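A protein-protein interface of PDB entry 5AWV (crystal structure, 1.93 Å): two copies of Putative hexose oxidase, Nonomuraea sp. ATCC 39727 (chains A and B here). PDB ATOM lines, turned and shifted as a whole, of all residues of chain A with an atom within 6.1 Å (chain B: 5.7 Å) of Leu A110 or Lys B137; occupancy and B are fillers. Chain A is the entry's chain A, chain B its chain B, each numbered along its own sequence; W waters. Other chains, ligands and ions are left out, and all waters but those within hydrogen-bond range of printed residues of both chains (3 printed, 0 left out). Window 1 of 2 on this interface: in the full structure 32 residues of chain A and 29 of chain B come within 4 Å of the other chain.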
ATOM      1  N   ALA A  30     -17.720   9.125  20.263  1.00  0.00           N
ATOM      2  CA  ALA A  30     -16.292   9.388  20.129  1.00  0.00           C
ATOM      3  C   ALA A  30     -15.507   8.048  19.987  1.00  0.00           C
ATOM      4  O   ALA A  30     -16.060   6.972  20.144  1.00  0.00           O
ATOM      5  CB  ALA A  30     -15.846  10.143  21.348  1.00  0.00           C
ATOM      6  N   GLY A  31     -14.239   8.160  19.632  1.00  0.00           N
ATOM      7  CA  GLY A  31     -13.329   7.048  19.418  1.00  0.00           C
ATOM      8  C   GLY A  31     -13.527   6.312  18.097  1.00  0.00           C
ATOM      9  O   GLY A  31     -14.420   6.648  17.356  1.00  0.00           O
ATOM     10  N   VAL A  33      -9.539   5.434  19.498  1.00  0.00           N
ATOM     11  CA  VAL A  33      -8.264   5.986  19.287  1.00  0.00           C
ATOM     12  C   VAL A  33      -7.212   5.015  19.812  1.00  0.00           C
ATOM     13  O   VAL A  33      -7.199   4.670  20.994  1.00  0.00           O
ATOM     14  CB  VAL A  33      -8.047   7.348  20.016  1.00  0.00           C
ATOM     15  CG1 VAL A  33      -6.792   8.023  19.518  1.00  0.00           C
ATOM     16  CG2 VAL A  33      -9.254   8.274  19.865  1.00  0.00           C
ATOM     17  N   LEU A  63      -8.519   3.927  23.416  1.00  0.00           N
ATOM     18  CA  LEU A  63      -9.705   4.664  23.858  1.00  0.00           C
ATOM     19  C   LEU A  63     -10.895   4.250  23.082  1.00  0.00           C
ATOM     20  O   LEU A  63     -10.852   4.250  21.836  1.00  0.00           O
ATOM     21  CB  LEU A  63      -9.497   6.172  23.628  1.00  0.00           C
ATOM     22  CG  LEU A  63      -8.573   6.831  24.616  1.00  0.00           C
ATOM     23  CD1 LEU A  63      -8.145   8.229  24.151  1.00  0.00           C
ATOM     24  CD2 LEU A  63      -9.162   6.933  26.034  1.00  0.00           C
ATOM     25  N   VAL A  64     -11.959   3.875  23.790  1.00  0.00           N
ATOM     26  CA  VAL A  64     -13.114   3.355  23.167  1.00  0.00           C
ATOM     27  C   VAL A  64     -14.381   4.133  23.616  1.00  0.00           C
ATOM     28  O   VAL A  64     -14.559   4.398  24.778  1.00  0.00           O
ATOM     29  CB  VAL A  64     -13.269   1.852  23.483  1.00  0.00           C
ATOM     30  CG1 VAL A  64     -12.157   1.053  22.848  1.00  0.00           C
ATOM     31  CG2 VAL A  64     -13.328   1.580  24.997  1.00  0.00           C
ATOM     32  N   GLY A  65     -15.237   4.466  22.667  1.00  0.00           N
ATOM     33  CA  GLY A  65     -16.459   5.254  22.881  1.00  0.00           C
ATOM     34  C   GLY A  65     -17.750   4.541  22.659  1.00  0.00           C
ATOM     35  O   GLY A  65     -18.820   5.151  22.769  1.00  0.00           O
ATOM     36  N   GLN A  69     -16.867  -0.662  19.603  1.00  0.00           N
ATOM     37  CA  GLN A  69     -15.486  -0.411  19.672  1.00  0.00           C
ATOM     38  C   GLN A  69     -14.750  -1.239  20.711  1.00  0.00           C
ATOM     39  O   GLN A  69     -13.581  -1.636  20.489  1.00  0.00           O
ATOM     40  CB  GLN A  69     -15.238   1.054  20.014  1.00  0.00           C
ATOM     41  CG  GLN A  69     -15.462   2.007  18.836  1.00  0.00           C
ATOM     42  CD  GLN A  69     -15.360   3.472  19.300  1.00  0.00           C
ATOM     43  OE1 GLN A  69     -14.445   3.836  19.999  1.00  0.00           O
ATOM     44  NE2 GLN A  69     -16.300   4.266  18.928  1.00  0.00           N
ATOM     45  N   ASP A 107      -8.984   1.678  27.689  1.00  0.00           N
ATOM     46  CA  ASP A 107      -9.263   2.769  28.591  1.00  0.00           C
ATOM     47  C   ASP A 107     -10.688   3.234  28.347  1.00  0.00           C
ATOM     48  O   ASP A 107     -11.046   3.583  27.227  1.00  0.00           O
ATOM     49  CB  ASP A 107      -8.250   3.896  28.396  1.00  0.00           C
ATOM     50  CG  ASP A 107      -8.419   5.025  29.441  1.00  0.00           C
ATOM     51  OD1 ASP A 107      -9.573   5.506  29.611  1.00  0.00           O
ATOM     52  OD2 ASP A 107      -7.413   5.350  30.111  1.00  0.00           O
ATOM     53  N   MET A 108     -11.512   3.218  29.392  1.00  0.00           N
ATOM     54  CA  MET A 108     -12.947   3.498  29.284  1.00  0.00           C
ATOM     55  C   MET A 108     -13.385   4.931  29.517  1.00  0.00           C
ATOM     56  O   MET A 108     -14.624   5.200  29.610  1.00  0.00           O
ATOM     57  CB  MET A 108     -13.724   2.609  30.221  1.00  0.00           C
ATOM     58  CG  MET A 108     -13.383   1.104  30.142  1.00  0.00           C
ATOM     59  SD  MET A 108     -13.690   0.261  28.572  1.00  0.00           S
ATOM     60  CE  MET A 108     -15.315  -0.266  28.909  1.00  0.00           C
ATOM     61  N   SER A 109     -12.427   5.828  29.539  1.00  0.00           N
ATOM     62  CA  SER A 109     -12.606   7.262  29.853  1.00  0.00           C
ATOM     63  C   SER A 109     -13.748   7.928  29.063  1.00  0.00           C
ATOM     64  O   SER A 109     -14.462   8.820  29.602  1.00  0.00           O
ATOM     65  CB  SER A 109     -11.358   8.058  29.504  1.00  0.00           C
ATOM     66  OG  SER A 109     -10.252   7.869  30.333  1.00  0.00           O
ATOM     67  N   LEU A 110     -13.907   7.543  27.796  1.00  0.00           N
ATOM     68  CA  LEU A 110     -14.974   8.119  26.968  1.00  0.00           C
ATOM     69  C   LEU A 110     -16.360   7.569  27.266  1.00  0.00           C
ATOM     70  O   LEU A 110     -17.333   8.182  26.822  1.00  0.00           O
ATOM     71  CB  LEU A 110     -14.627   7.980  25.480  1.00  0.00           C
ATOM     72  CG  LEU A 110     -13.359   8.654  24.958  1.00  0.00           C
ATOM     73  CD1 LEU A 110     -13.147   8.305  23.510  1.00  0.00           C
ATOM     74  CD2 LEU A 110     -13.405  10.163  25.059  1.00  0.00           C
ATOM     75  N   LEU A 111     -16.494   6.450  28.008  1.00  0.00           N
ATOM     76  CA  LEU A 111     -17.822   5.867  28.275  1.00  0.00           C
ATOM     77  C   LEU A 111     -18.452   6.341  29.523  1.00  0.00           C
ATOM     78  O   LEU A 111     -18.308   5.683  30.553  1.00  0.00           O
ATOM     79  CB  LEU A 111     -17.729   4.337  28.346  1.00  0.00           C
ATOM     80  CG  LEU A 111     -17.432   3.623  27.012  1.00  0.00           C
ATOM     81  CD1 LEU A 111     -17.039   2.146  27.153  1.00  0.00           C
ATOM     82  CD2 LEU A 111     -18.593   3.729  26.008  1.00  0.00           C
ATOM     83  N   THR A 112     -19.207   7.433  29.467  1.00  0.00           N
ATOM     84  CA  THR A 112     -19.636   8.147  30.670  1.00  0.00           C
ATOM     85  C   THR A 112     -21.163   8.452  30.709  1.00  0.00           C
ATOM     86  O   THR A 112     -21.582   9.373  31.374  1.00  0.00           O
ATOM     87  CB  THR A 112     -18.895   9.484  30.830  1.00  0.00           C
ATOM     88  OG1 THR A 112     -19.173  10.281  29.692  1.00  0.00           O
ATOM     89  CG2 THR A 112     -17.454   9.324  30.953  1.00  0.00           C
ATOM     90  N   GLU A 113     -21.993   7.722  29.995  1.00  0.00           N
ATOM     91  CA  GLU A 113     -23.445   7.977  30.097  1.00  0.00           C
ATOM     92  C   GLU A 113     -24.040   7.608  31.485  1.00  0.00           C
ATOM     93  O   GLU A 113     -23.648   6.608  32.091  1.00  0.00           O
ATOM     94  CB  GLU A 113     -24.176   7.175  29.008  1.00  0.00           C
ATOM     95  CG  GLU A 113     -25.700   7.185  29.162  1.00  0.00           C
ATOM     96  CD  GLU A 113     -26.446   7.561  27.911  1.00  0.00           C
ATOM     97  OE1 GLU A 113     -27.141   6.677  27.328  1.00  0.00           O
ATOM     98  OE2 GLU A 113     -26.360   8.766  27.559  1.00  0.00           O
ATOM     99  N   GLU A 126     -22.474   3.949  32.794  1.00  0.00           N
ATOM    100  CA  GLU A 126     -21.316   3.462  32.073  1.00  0.00           C
ATOM    101  C   GLU A 126     -20.050   3.470  32.925  1.00  0.00           C
ATOM    102  O   GLU A 126     -19.985   4.253  33.861  1.00  0.00           O
ATOM    103  CB  GLU A 126     -21.130   4.239  30.741  1.00  0.00           C
ATOM    104  CG  GLU A 126     -22.085   3.730  29.701  1.00  0.00           C
ATOM    105  CD  GLU A 126     -21.954   4.384  28.345  1.00  0.00           C
ATOM    106  OE1 GLU A 126     -21.389   5.473  28.243  1.00  0.00           O
ATOM    107  OE2 GLU A 126     -22.466   3.783  27.373  1.00  0.00           O
ATOM    108  N   GLY A 128     -16.833   4.242  32.608  1.00  0.00           N
ATOM    109  CA  GLY A 128     -15.875   5.320  32.686  1.00  0.00           C
ATOM    110  C   GLY A 128     -16.246   6.478  33.584  1.00  0.00           C
ATOM    111  O   GLY A 128     -15.395   7.365  33.845  1.00  0.00           O
ATOM    112  N   ILE B 114     -20.611  16.776  24.834  1.00  0.00           N
ATOM    113  CA  ILE B 114     -19.472  17.215  24.018  1.00  0.00           C
ATOM    114  C   ILE B 114     -19.266  16.149  22.914  1.00  0.00           C
ATOM    115  O   ILE B 114     -19.011  14.982  23.236  1.00  0.00           O
ATOM    116  CB  ILE B 114     -18.220  17.338  24.820  1.00  0.00           C
ATOM    117  CG1 ILE B 114     -18.346  18.390  25.958  1.00  0.00           C
ATOM    118  CG2 ILE B 114     -17.058  17.751  23.892  1.00  0.00           C
ATOM    119  CD1 ILE B 114     -17.353  18.213  27.092  1.00  0.00           C
ATOM    120  N   ALA B 115     -19.433  16.519  21.630  1.00  0.00           N
ATOM    121  CA  ALA B 115     -19.327  15.552  20.573  1.00  0.00           C
ATOM    122  C   ALA B 115     -19.036  16.185  19.248  1.00  0.00           C
ATOM    123  O   ALA B 115     -19.387  17.378  18.995  1.00  0.00           O
ATOM    124  CB  ALA B 115     -20.606  14.781  20.486  1.00  0.00           C
ATOM    125  N   SER B 132     -12.954  22.602  32.248  1.00  0.00           N
ATOM    126  CA  SER B 132     -12.099  21.474  32.474  1.00  0.00           C
ATOM    127  C   SER B 132     -12.664  20.195  31.834  1.00  0.00           C
ATOM    128  O   SER B 132     -11.871  19.480  31.231  1.00  0.00           O
ATOM    129  CB  SER B 132     -11.800  21.346  33.972  1.00  0.00           C
ATOM    130  OG  SER B 132     -12.919  20.788  34.565  1.00  0.00           O
ATOM    131  N   GLU B 133     -14.011  19.976  31.806  1.00  0.00           N
ATOM    132  CA  GLU B 133     -14.627  18.851  31.079  1.00  0.00           C
ATOM    133  C   GLU B 133     -14.423  18.957  29.581  1.00  0.00           C
ATOM    134  O   GLU B 133     -14.122  17.944  28.942  1.00  0.00           O
ATOM    135  CB  GLU B 133     -16.137  18.725  31.325  1.00  0.00           C
ATOM    136  CG  GLU B 133     -16.428  18.429  32.782  1.00  0.00           C
ATOM    137  CD  GLU B 133     -17.907  18.700  33.184  1.00  0.00           C
ATOM    138  OE1 GLU B 133     -18.593  19.640  32.680  1.00  0.00           O
ATOM    139  OE2 GLU B 133     -18.376  17.952  34.065  1.00  0.00           O
ATOM    140  N   VAL B 134     -14.441  20.190  29.050  1.00  0.00           N
ATOM    141  CA  VAL B 134     -14.274  20.412  27.634  1.00  0.00           C
ATOM    142  C   VAL B 134     -12.859  20.099  27.256  1.00  0.00           C
ATOM    143  O   VAL B 134     -12.658  19.422  26.276  1.00  0.00           O
ATOM    144  CB  VAL B 134     -14.564  21.888  27.245  1.00  0.00           C
ATOM    145  CG1 VAL B 134     -14.090  22.204  25.828  1.00  0.00           C
ATOM    146  CG2 VAL B 134     -16.060  22.216  27.398  1.00  0.00           C
ATOM    147  N   TYR B 135     -11.892  20.638  27.990  1.00  0.00           N
ATOM    148  CA  TYR B 135     -10.488  20.439  27.637  1.00  0.00           C
ATOM    149  C   TYR B 135     -10.140  18.931  27.674  1.00  0.00           C
ATOM    150  O   TYR B 135      -9.482  18.470  26.774  1.00  0.00           O
ATOM    151  CB  TYR B 135      -9.531  21.189  28.534  1.00  0.00           C
ATOM    152  CG  TYR B 135      -9.707  22.712  28.483  1.00  0.00           C
ATOM    153  CD1 TYR B 135     -10.096  23.366  27.304  1.00  0.00           C
ATOM    154  CD2 TYR B 135      -9.494  23.441  29.608  1.00  0.00           C
ATOM    155  CE1 TYR B 135     -10.196  24.752  27.257  1.00  0.00           C
ATOM    156  CE2 TYR B 135      -9.633  24.818  29.607  1.00  0.00           C
ATOM    157  CZ  TYR B 135     -10.009  25.464  28.437  1.00  0.00           C
ATOM    158  OH  TYR B 135     -10.155  26.853  28.439  1.00  0.00           O
ATOM    159  N   GLU B 136     -10.606  18.224  28.662  1.00  0.00           N
ATOM    160  CA  GLU B 136     -10.313  16.775  28.747  1.00  0.00           C
ATOM    161  C   GLU B 136     -10.876  15.948  27.631  1.00  0.00           C
ATOM    162  O   GLU B 136     -10.164  15.096  27.073  1.00  0.00           O
ATOM    163  CB  GLU B 136     -10.814  16.145  30.027  1.00  0.00           C
ATOM    164  CG  GLU B 136      -9.984  16.409  31.224  1.00  0.00           C
ATOM    165  CD  GLU B 136      -8.631  15.677  31.231  1.00  0.00           C
ATOM    166  OE1 GLU B 136      -8.305  14.741  30.415  1.00  0.00           O
ATOM    167  OE2 GLU B 136      -7.919  16.127  32.142  1.00  0.00           O
ATOM    168  N   LYS B 137     -12.158  16.164  27.337  1.00  0.00           N
ATOM    169  CA  LYS B 137     -12.871  15.395  26.341  1.00  0.00           C
ATOM    170  C   LYS B 137     -12.361  15.700  24.931  1.00  0.00           C
ATOM    171  O   LYS B 137     -12.122  14.803  24.150  1.00  0.00           O
ATOM    172  CB  LYS B 137     -14.391  15.658  26.445  1.00  0.00           C
ATOM    173  CG  LYS B 137     -15.333  14.480  26.297  1.00  0.00           C
ATOM    174  CD  LYS B 137     -15.383  13.912  24.959  1.00  0.00           C
ATOM    175  CE  LYS B 137     -16.334  12.740  24.911  1.00  0.00           C
ATOM    176  NZ  LYS B 137     -17.763  13.047  25.109  1.00  0.00           N
ATOM    177  N   LEU B 138     -12.164  16.969  24.628  1.00  0.00           N
ATOM    178  CA  LEU B 138     -11.582  17.354  23.320  1.00  0.00           C
ATOM    179  C   LEU B 138     -10.185  16.812  23.114  1.00  0.00           C
ATOM    180  O   LEU B 138      -9.847  16.435  22.004  1.00  0.00           O
ATOM    181  CB  LEU B 138     -11.570  18.882  23.101  1.00  0.00           C
ATOM    182  CG  LEU B 138     -12.908  19.567  22.971  1.00  0.00           C
ATOM    183  CD1 LEU B 138     -12.726  21.072  22.848  1.00  0.00           C
ATOM    184  CD2 LEU B 138     -13.738  18.944  21.843  1.00  0.00           C
ATOM    185  N   TYR B 139      -9.410  16.790  24.169  1.00  0.00           N
ATOM    186  CA  TYR B 139      -8.092  16.296  24.121  1.00  0.00           C
ATOM    187  C   TYR B 139      -8.042  14.786  23.933  1.00  0.00           C
ATOM    188  O   TYR B 139      -7.386  14.316  22.997  1.00  0.00           O
ATOM    189  CB  TYR B 139      -7.307  16.663  25.366  1.00  0.00           C
ATOM    190  CG  TYR B 139      -5.823  16.278  25.318  1.00  0.00           C
ATOM    191  CD1 TYR B 139      -5.015  16.564  24.215  1.00  0.00           C
ATOM    192  CD2 TYR B 139      -5.207  15.630  26.396  1.00  0.00           C
ATOM    193  CE1 TYR B 139      -3.624  16.259  24.230  1.00  0.00           C
ATOM    194  CE2 TYR B 139      -3.824  15.341  26.410  1.00  0.00           C
ATOM    195  CZ  TYR B 139      -3.044  15.669  25.318  1.00  0.00           C
ATOM    196  OH  TYR B 139      -1.682  15.339  25.335  1.00  0.00           O
ATOM    197  N   LEU B 140      -8.720  14.050  24.780  1.00  0.00           N
ATOM    198  CA  LEU B 140      -8.751  12.576  24.652  1.00  0.00           C
ATOM    199  C   LEU B 140      -9.359  12.106  23.344  1.00  0.00           C
ATOM    200  O   LEU B 140      -8.792  11.233  22.672  1.00  0.00           O
ATOM    201  CB  LEU B 140      -9.537  11.961  25.803  1.00  0.00           C
ATOM    202  CG  LEU B 140      -8.802  12.114  27.151  1.00  0.00           C
ATOM    203  CD1 LEU B 140      -9.526  11.314  28.218  1.00  0.00           C
ATOM    204  CD2 LEU B 140      -7.346  11.629  27.085  1.00  0.00           C
ATOM    205  N   GLY B 141     -10.477  12.688  22.946  1.00  0.00           N
ATOM    206  CA  GLY B 141     -11.185  12.222  21.812  1.00  0.00           C
ATOM    207  C   GLY B 141     -10.464  12.503  20.495  1.00  0.00           C
ATOM    208  O   GLY B 141     -10.527  11.693  19.598  1.00  0.00           O
ATOM    209  N   TRP B 142      -9.877  13.700  20.374  1.00  0.00           N
ATOM    210  CA  TRP B 142      -9.457  14.244  19.096  1.00  0.00           C
ATOM    211  C   TRP B 142      -8.159  14.976  19.058  1.00  0.00           C
ATOM    212  O   TRP B 142      -7.751  15.390  17.982  1.00  0.00           O
ATOM    213  CB  TRP B 142     -10.566  15.131  18.499  1.00  0.00           C
ATOM    214  CG  TRP B 142     -11.867  14.453  18.352  1.00  0.00           C
ATOM    215  CD1 TRP B 142     -12.273  13.712  17.291  1.00  0.00           C
ATOM    216  CD2 TRP B 142     -12.941  14.409  19.287  1.00  0.00           C
ATOM    217  NE1 TRP B 142     -13.510  13.202  17.507  1.00  0.00           N
ATOM    218  CE2 TRP B 142     -13.938  13.597  18.733  1.00  0.00           C
ATOM    219  CE3 TRP B 142     -13.153  14.959  20.544  1.00  0.00           C
ATOM    220  CZ2 TRP B 142     -15.164  13.386  19.357  1.00  0.00           C
ATOM    221  CZ3 TRP B 142     -14.326  14.703  21.172  1.00  0.00           C
ATOM    222  CH2 TRP B 142     -15.320  13.922  20.592  1.00  0.00           C
HETATM  223  O   HOH W   1     -17.268  11.011  27.349  1.00  0.00           O
HETATM  224  O   HOH W   2     -12.653  10.222  18.731  1.00  0.00           O
HETATM  225  O   HOH W   3     -17.700   9.844  24.397  1.00  0.00           O
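Trp B142 touches Ala A30 (CZ2 to CB, 3.9 Å).
O of Gly B141 touches CG2 of Val A33 (3.7 Å).
O of Leu B140 touches CD1 of Leu A63 (3.4 Å).
Ser A109 touches Leu B140.
Leu A110 touches Lys B137.
No position is printed for both chains.
Of the 5 pairs that touch across the chains among the printed residues, none has its exchanged pair printed and touching as well.
Printed residues of chain B within 4 Å of Leu A63: Leu B140 (3.4 Å).
Of the printed residues of chain B, Ser A109 touches Leu B140.
Of chain B, only Lys B137 comes within 4 Å of Leu A110.
Glu A113 touches none of the printed residues of chain B.
Lys B137 touches just one residue of chain A: Leu A110.
Printed residues of chain A within 4 Å of Leu B140: Leu A63 and Ser A109.
Printed residues of chain A within 4 Å of Trp B142: Ala A30 (3.9 Å).
The nearest residue of chain B that does not touch Leu A110 is Leu B140 (4.3 Å).
The nearest printed residue of chain B that does not touch Leu A63 is Gly B141 (5.2 Å).
Water W2 lies within hydrogen-bond range of the backbone carbonyl oxygen of Gly B141 (2.7 Å), the backbone NH of Gly A31 (2.8 Å) and the indole nitrogen of Trp B142 (3.3 Å).
Water W1 lies within hydrogen-bond range of O of Leu A110, NZ of Lys B137 and OG1 of Thr A112.
Water W3 lies within hydrogen-bond range of the backbone carbonyl oxygen (O) of Leu A110 (3.0 Å) and the side-chain amino group (NZ) of Lys B137 (3.3 Å).
NE2 of Gln A69 sits at hydrogen-bond distance from O of Ala A30, 3.0 Å away.
The backbone carbonyl oxygen (O) of Val A33 sits at hydrogen-bond distance from the backbone NH (N) of Leu A63 (2.9 Å).
The side-chain carboxylate (OD1) of Asp A107 is in hydrogen-bond range of the side-chain hydroxyl (OG) of Ser A109 (2.6 Å).
The backbone carbonyl oxygen (O) of Ile B114 sits at hydrogen-bond distance from the side-chain amino group (NZ) of Lys B137 (3.0 Å).
Hydrophobic or aromatic side chains of chain B within 4 Å of the printed part of chain A: Leu B140 and Trp B142.
Of the 16 printed residues of chain A, 5 touch a printed residue of chain B.
Hydrophobic or aromatic side chains of chain A that line the printed part of chain B: Ala A30, Val A33, Leu A63 and Leu A110.
Among the printed residues, no Asp or Glu carboxylate lies within 4 Å of a Lys or Arg side-chain nitrogen of the other chain.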
